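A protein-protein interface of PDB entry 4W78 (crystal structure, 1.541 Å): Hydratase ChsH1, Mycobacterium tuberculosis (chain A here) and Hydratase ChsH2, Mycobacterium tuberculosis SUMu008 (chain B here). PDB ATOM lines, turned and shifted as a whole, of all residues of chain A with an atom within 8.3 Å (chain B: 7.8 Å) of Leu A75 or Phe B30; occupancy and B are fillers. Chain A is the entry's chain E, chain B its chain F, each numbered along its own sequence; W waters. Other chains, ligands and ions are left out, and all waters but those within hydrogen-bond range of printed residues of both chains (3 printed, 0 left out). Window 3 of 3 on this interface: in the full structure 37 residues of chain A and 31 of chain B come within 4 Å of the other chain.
The backbone carbonyl oxygen (O) of Met A72 sits at hydrogen-bond distance from the guanidinium group (NH2) of Arg B28 (3.0 Å).
The backbone carbonyl oxygen (O) of Ala B24 sits at hydrogen-bond distance from the side-chain hydroxyl (OG1) of Thr B27 (2.8 Å).
The side-chain carboxylate (OD1) of Asp B29 is in hydrogen-bond range of the backbone NH (N) of Gln B31, 3.0 Å away.
OG1 of Thr B27 lies within hydrogen-bond range of ND2 of Asn B51 (2.9 Å).
O of Ala B24 sits at hydrogen-bond distance from N of Asp B29 (3.0 Å).
OD2 of Asp B29 sits close to ND2 of Asn B51, at 2.8 Å.
Arg B28 touches Arg A24.
Thr B27 touches Met A72 (O to CG, 3.5 Å).
CE of Met A72 touches CA of Asp B29 (3.9 Å).
Arg B28 touches Met A73.
Arg B28 touches Gly A74 (NH2 to N, 3.9 Å).
CA of Gly A74 touches CD1 of Phe B30 (3.6 Å).
Leu A75 touches Phe B30 (CG to CD2, 3.7 Å).
Of the printed residues of chain B, Met A73 touches Arg B28 (3.7 Å).
Of chain B, only Arg B28 (3.9 Å) and Phe B30 (3.6 Å) come within 4 Å of Gly A74.
Leu A75 touches one residue of chain B.
Gly A77 touches none of the printed residues of chain B.
Of the printed residues of chain A, Thr B27 touches Met A72 (3.5 Å).
Printed residues of chain A within 4 Å of Arg B28: Arg A24 (3.7 Å), Met A72 (3.0 Å), Met A73 (3.7 Å) and Gly A74 (3.9 Å).
Of the printed residues of chain A, Asp B29 touches Met A72 (3.9 Å).
Val B33 touches none of the printed residues of chain A.
The nearest residue of chain A that does not touch Phe B30 is Met A72 (5.6 Å).
The nearest printed residue of chain B that does not touch Met A73 is Phe B30 (6.0 Å).
Hydrophobic or aromatic side chains of chain B that line the printed part of chain A: Phe B30.
Along chain B the printed residues that touch a printed residue of chain A span positions 27 to 30.
Hydrophobic or aromatic side chains of chain A that line the printed part of chain B: Met A72 and Leu A75.
Among the printed residues, no Asp or Glu carboxylate lies within 4 Å of a Lys or Arg side-chain nitrogen of the other chain.
Water W3 lies within hydrogen-bond range of the backbone carbonyl oxygen of Met A73 (2.6 Å), the guanidinium group of Arg B28 (2.6 Å) and the guanidinium group of Arg A24 (3.4 Å).
Water W2 lies within hydrogen-bond range of O of Arg B28 (2.7 Å) and N of Gly A74 (2.8 Å).
Water W1 bridges the guanidinium group (NE) of Arg B28 and the guanidinium group (NH1) of Arg A24.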
ATOM      1  N   ARG A  24      24.787  34.586   7.176  1.00  0.00           N
ATOM      2  CA  ARG A  24      25.662  33.681   6.440  1.00  0.00           C
ATOM      3  C   ARG A  24      25.792  34.090   4.976  1.00  0.00           C
ATOM      4  O   ARG A  24      26.879  34.051   4.401  1.00  0.00           O
ATOM      5  CB  ARG A  24      25.134  32.242   6.527  1.00  0.00           C
ATOM      6  CG  ARG A  24      26.043  31.229   5.864  1.00  0.00           C
ATOM      7  CD  ARG A  24      25.402  29.846   5.760  1.00  0.00           C
ATOM      8  NE  ARG A  24      24.305  29.896   4.803  1.00  0.00           N
ATOM      9  CZ  ARG A  24      23.513  28.881   4.489  1.00  0.00           C
ATOM     10  NH1 ARG A  24      23.664  27.711   5.076  1.00  0.00           N
ATOM     11  NH2 ARG A  24      22.544  29.071   3.585  1.00  0.00           N
ATOM     12  N   MET A  72      19.516  33.013  10.603  1.00  0.00           N
ATOM     13  CA  MET A  72      19.438  31.736  11.323  1.00  0.00           C
ATOM     14  C   MET A  72      20.817  31.068  11.315  1.00  0.00           C
ATOM     15  O   MET A  72      21.585  31.206  10.374  1.00  0.00           O
ATOM     16  CB  MET A  72      18.404  30.811  10.675  1.00  0.00           C
ATOM     17  CG  MET A  72      16.962  31.308  10.770  1.00  0.00           C
ATOM     18  SD  MET A  72      16.308  31.484  12.441  1.00  0.00           S
ATOM     19  CE  MET A  72      15.689  29.830  12.694  1.00  0.00           C
ATOM     20  N   MET A  73      21.113  30.326  12.379  1.00  0.00           N
ATOM     21  CA  MET A  73      22.367  29.594  12.462  1.00  0.00           C
ATOM     22  C   MET A  73      22.404  28.400  11.515  1.00  0.00           C
ATOM     23  O   MET A  73      23.451  28.059  10.966  1.00  0.00           O
ATOM     24  CB  MET A  73      22.573  29.113  13.896  1.00  0.00           C
ATOM     25  CG  MET A  73      22.949  30.216  14.843  1.00  0.00           C
ATOM     26  SD  MET A  73      24.658  30.723  14.590  1.00  0.00           S
ATOM     27  CE  MET A  73      24.654  32.259  15.504  1.00  0.00           C
ATOM     28  N   GLY A  74      21.256  27.765  11.324  1.00  0.00           N
ATOM     29  CA  GLY A  74      21.191  26.554  10.516  1.00  0.00           C
ATOM     30  C   GLY A  74      21.964  25.405  11.150  1.00  0.00           C
ATOM     31  O   GLY A  74      22.163  25.373  12.366  1.00  0.00           O
ATOM     32  N   LEU A  75      22.411  24.452  10.338  1.00  0.00           N
ATOM     33  CA  LEU A  75      23.163  23.319  10.871  1.00  0.00           C
ATOM     34  C   LEU A  75      24.627  23.625  11.153  1.00  0.00           C
ATOM     35  O   LEU A  75      25.201  23.094  12.105  1.00  0.00           O
ATOM     36  CB  LEU A  75      23.093  22.124   9.924  1.00  0.00           C
ATOM     37  CG  LEU A  75      21.738  21.446   9.789  1.00  0.00           C
ATOM     38  CD1 LEU A  75      21.847  20.350   8.743  1.00  0.00           C
ATOM     39  CD2 LEU A  75      21.290  20.855  11.113  1.00  0.00           C
ATOM     40  N   GLY A  76      25.235  24.462  10.318  1.00  0.00           N
ATOM     41  CA  GLY A  76      26.668  24.707  10.405  1.00  0.00           C
ATOM     42  C   GLY A  76      27.070  25.922  11.219  1.00  0.00           C
ATOM     43  O   GLY A  76      28.248  26.096  11.551  1.00  0.00           O
ATOM     44  N   GLY A  77      26.100  26.764  11.557  1.00  0.00           N
ATOM     45  CA  GLY A  77      26.383  27.965  12.323  1.00  0.00           C
ATOM     46  C   GLY A  77      26.835  27.680  13.742  1.00  0.00           C
ATOM     47  O   GLY A  77      26.264  26.834  14.431  1.00  0.00           O
ATOM     48  N   VAL A  78      27.876  28.383  14.177  1.00  0.00           N
ATOM     49  CA  VAL A  78      28.318  28.320  15.563  1.00  0.00           C
ATOM     50  C   VAL A  78      27.944  29.622  16.273  1.00  0.00           C
ATOM     51  O   VAL A  78      28.339  30.708  15.846  1.00  0.00           O
ATOM     52  CB  VAL A  78      29.837  28.057  15.670  1.00  0.00           C
ATOM     53  CG1 VAL A  78      30.619  28.955  14.712  1.00  0.00           C
ATOM     54  CG2 VAL A  78      30.311  28.236  17.102  1.00  0.00           C
ATOM     55  N   ALA B  24       9.597  24.585   7.377  1.00  0.00           N
ATOM     56  CA  ALA B  24      10.565  24.763   8.447  1.00  0.00           C
ATOM     57  C   ALA B  24      11.974  24.897   7.897  1.00  0.00           C
ATOM     58  O   ALA B  24      12.694  25.828   8.283  1.00  0.00           O
ATOM     59  CB  ALA B  24      10.491  23.608   9.451  1.00  0.00           C
ATOM     60  N   LEU B  25      12.375  24.003   6.997  1.00  0.00           N
ATOM     61  CA  LEU B  25      13.749  24.053   6.493  1.00  0.00           C
ATOM     62  C   LEU B  25      13.997  25.240   5.561  1.00  0.00           C
ATOM     63  O   LEU B  25      15.110  25.766   5.535  1.00  0.00           O
ATOM     64  CB  LEU B  25      14.204  22.724   5.869  1.00  0.00           C
ATOM     65  CG  LEU B  25      14.815  21.774   6.903  1.00  0.00           C
ATOM     66  CD1 LEU B  25      13.832  21.344   7.986  1.00  0.00           C
ATOM     67  CD2 LEU B  25      15.426  20.584   6.204  1.00  0.00           C
ATOM     68  N   ALA B  26      12.967  25.671   4.834  1.00  0.00           N
ATOM     69  CA  ALA B  26      13.112  26.860   3.993  1.00  0.00           C
ATOM     70  C   ALA B  26      13.234  28.120   4.845  1.00  0.00           C
ATOM     71  O   ALA B  26      13.720  29.150   4.365  1.00  0.00           O
ATOM     72  CB  ALA B  26      11.936  26.994   3.009  1.00  0.00           C
ATOM     73  N   THR B  27      12.774  28.071   6.096  1.00  0.00           N
ATOM     74  CA  THR B  27      12.998  29.207   7.002  1.00  0.00           C
ATOM     75  C   THR B  27      14.296  29.016   7.795  1.00  0.00           C
ATOM     76  O   THR B  27      14.594  29.794   8.699  1.00  0.00           O
ATOM     77  CB  THR B  27      11.829  29.455   7.982  1.00  0.00           C
ATOM     78  OG1 THR B  27      11.721  28.345   8.891  1.00  0.00           O
ATOM     79  CG2 THR B  27      10.509  29.614   7.252  1.00  0.00           C
ATOM     80  N   ARG B  28      15.049  27.975   7.437  1.00  0.00           N
ATOM     81  CA  ARG B  28      16.331  27.636   8.063  1.00  0.00           C
ATOM     82  C   ARG B  28      16.228  27.342   9.569  1.00  0.00           C
ATOM     83  O   ARG B  28      17.143  27.611  10.357  1.00  0.00           O
ATOM     84  CB  ARG B  28      17.411  28.677   7.755  1.00  0.00           C
ATOM     85  CG  ARG B  28      17.715  28.780   6.266  1.00  0.00           C
ATOM     86  CD  ARG B  28      18.891  29.694   6.002  1.00  0.00           C
ATOM     87  NE  ARG B  28      20.123  29.237   6.638  1.00  0.00           N
ATOM     88  CZ  ARG B  28      20.920  30.025   7.351  1.00  0.00           C
ATOM     89  NH1 ARG B  28      20.599  31.304   7.514  1.00  0.00           N
ATOM     90  NH2 ARG B  28      22.035  29.549   7.902  1.00  0.00           N
ATOM     91  N   ASP B  29      15.086  26.758   9.930  1.00  0.00           N
ATOM     92  CA  ASP B  29      14.800  26.308  11.280  1.00  0.00           C
ATOM     93  C   ASP B  29      14.933  24.797  11.305  1.00  0.00           C
ATOM     94  O   ASP B  29      14.076  24.080  10.766  1.00  0.00           O
ATOM     95  CB  ASP B  29      13.375  26.723  11.634  1.00  0.00           C
ATOM     96  CG  ASP B  29      13.003  26.403  13.041  1.00  0.00           C
ATOM     97  OD1 ASP B  29      13.671  25.567  13.696  1.00  0.00           O
ATOM     98  OD2 ASP B  29      12.013  27.000  13.507  1.00  0.00           O
ATOM     99  N   PHE B  30      16.029  24.333  11.904  1.00  0.00           N
ATOM    100  CA  PHE B  30      16.346  22.911  11.952  1.00  0.00           C
ATOM    101  C   PHE B  30      15.994  22.274  13.284  1.00  0.00           C
ATOM    102  O   PHE B  30      16.430  21.163  13.586  1.00  0.00           O
ATOM    103  CB  PHE B  30      17.821  22.688  11.604  1.00  0.00           C
ATOM    104  CG  PHE B  30      18.135  22.980  10.170  1.00  0.00           C
ATOM    105  CD1 PHE B  30      18.465  24.261   9.771  1.00  0.00           C
ATOM    106  CD2 PHE B  30      18.071  21.970   9.211  1.00  0.00           C
ATOM    107  CE1 PHE B  30      18.724  24.540   8.427  1.00  0.00           C
ATOM    108  CE2 PHE B  30      18.337  22.234   7.886  1.00  0.00           C
ATOM    109  CZ  PHE B  30      18.662  23.521   7.495  1.00  0.00           C
ATOM    110  N   GLN B  31      15.185  22.969  14.077  1.00  0.00           N
ATOM    111  CA  GLN B  31      14.781  22.413  15.363  1.00  0.00           C
ATOM    112  C   GLN B  31      14.063  21.092  15.128  1.00  0.00           C
ATOM    113  O   GLN B  31      13.160  21.000  14.293  1.00  0.00           O
ATOM    114  CB  GLN B  31      13.878  23.384  16.142  1.00  0.00           C
ATOM    115  CG  GLN B  31      13.784  23.056  17.640  1.00  0.00           C
ATOM    116  CD  GLN B  31      15.045  23.430  18.431  1.00  0.00           C
ATOM    117  OE1 GLN B  31      15.804  24.324  18.029  1.00  0.00           O
ATOM    118  NE2 GLN B  31      15.271  22.750  19.551  1.00  0.00           N
ATOM    119  N   ASP B  32      14.469  20.068  15.871  1.00  0.00           N
ATOM    120  CA  ASP B  32      13.969  18.722  15.617  1.00  0.00           C
ATOM    121  C   ASP B  32      12.438  18.591  15.598  1.00  0.00           C
ATOM    122  O   ASP B  32      11.888  17.826  14.806  1.00  0.00           O
ATOM    123  CB  ASP B  32      14.634  17.710  16.567  1.00  0.00           C
ATOM    124  CG  ASP B  32      14.613  18.139  18.033  1.00  0.00           C
ATOM    125  OD1 ASP B  32      13.795  18.999  18.438  1.00  0.00           O
ATOM    126  OD2 ASP B  32      15.429  17.572  18.803  1.00  0.00           O
ATOM    127  N   VAL B  33      11.752  19.365  16.433  1.00  0.00           N
ATOM    128  CA  VAL B  33      10.307  19.225  16.587  1.00  0.00           C
ATOM    129  C   VAL B  33       9.501  19.529  15.318  1.00  0.00           C
ATOM    130  O   VAL B  33       8.319  19.177  15.246  1.00  0.00           O
ATOM    131  CB  VAL B  33       9.781  20.094  17.749  1.00  0.00           C
ATOM    132  CG1 VAL B  33      10.379  19.652  19.074  1.00  0.00           C
ATOM    133  CG2 VAL B  33      10.067  21.581  17.474  1.00  0.00           C
ATOM    134  N   HIS B  34      10.108  20.178  14.321  1.00  0.00           N
ATOM    135  CA  HIS B  34       9.358  20.470  13.101  1.00  0.00           C
ATOM    136  C   HIS B  34       9.526  19.411  12.015  1.00  0.00           C
ATOM    137  O   HIS B  34       8.856  19.477  10.979  1.00  0.00           O
ATOM    138  CB  HIS B  34       9.740  21.843  12.520  1.00  0.00           C
ATOM    139  CG  HIS B  34       9.748  22.937  13.535  1.00  0.00           C
ATOM    140  ND1 HIS B  34       8.639  23.274  14.287  1.00  0.00           N
ATOM    141  CD2 HIS B  34      10.745  23.747  13.951  1.00  0.00           C
ATOM    142  CE1 HIS B  34       8.957  24.243  15.124  1.00  0.00           C
ATOM    143  NE2 HIS B  34      10.229  24.537  14.946  1.00  0.00           N
ATOM    144  N   HIS B  35      10.413  18.437  12.225  1.00  0.00           N
ATOM    145  CA  HIS B  35      10.618  17.408  11.206  1.00  0.00           C
ATOM    146  C   HIS B  35      10.878  16.009  11.768  1.00  0.00           C
ATOM    147  O   HIS B  35      10.915  15.038  11.017  1.00  0.00           O
ATOM    148  CB  HIS B  35      11.768  17.792  10.278  1.00  0.00           C
ATOM    149  CG  HIS B  35      13.089  17.862  10.976  1.00  0.00           C
ATOM    150  ND1 HIS B  35      13.630  19.054  11.407  1.00  0.00           N
ATOM    151  CD2 HIS B  35      13.961  16.893  11.345  1.00  0.00           C
ATOM    152  CE1 HIS B  35      14.783  18.813  12.008  1.00  0.00           C
ATOM    153  NE2 HIS B  35      15.004  17.510  11.989  1.00  0.00           N
ATOM    154  N   ASP B  36      11.070  15.898  13.080  1.00  0.00           N
ATOM    155  CA  ASP B  36      11.351  14.619  13.710  1.00  0.00           C
ATOM    156  C   ASP B  36      10.202  14.326  14.674  1.00  0.00           C
ATOM    157  O   ASP B  36      10.138  14.889  15.764  1.00  0.00           O
ATOM    158  CB  ASP B  36      12.690  14.726  14.463  1.00  0.00           C
ATOM    159  CG  ASP B  36      13.115  13.432  15.146  1.00  0.00           C
ATOM    160  OD1 ASP B  36      12.265  12.559  15.417  1.00  0.00           O
ATOM    161  OD2 ASP B  36      14.328  13.295  15.441  1.00  0.00           O
ATOM    162  N   ASN B  51       6.405  25.775  12.398  1.00  0.00           N
ATOM    163  CA  ASN B  51       7.222  26.718  13.178  1.00  0.00           C
ATOM    164  C   ASN B  51       6.727  28.160  13.056  1.00  0.00           C
ATOM    165  O   ASN B  51       5.877  28.470  12.209  1.00  0.00           O
ATOM    166  CB  ASN B  51       8.719  26.612  12.817  1.00  0.00           C
ATOM    167  CG  ASN B  51       9.065  27.266  11.474  1.00  0.00           C
ATOM    168  OD1 ASN B  51       8.213  27.423  10.614  1.00  0.00           O
ATOM    169  ND2 ASN B  51      10.319  27.669  11.315  1.00  0.00           N
HETATM  170  O   HOH W   1      20.627  26.566   6.148  1.00  0.00           O
HETATM  171  O   HOH W   2      18.731  27.758  12.573  1.00  0.00           O
HETATM  172  O   HOH W   3      23.573  27.531   8.444  1.00  0.00           O
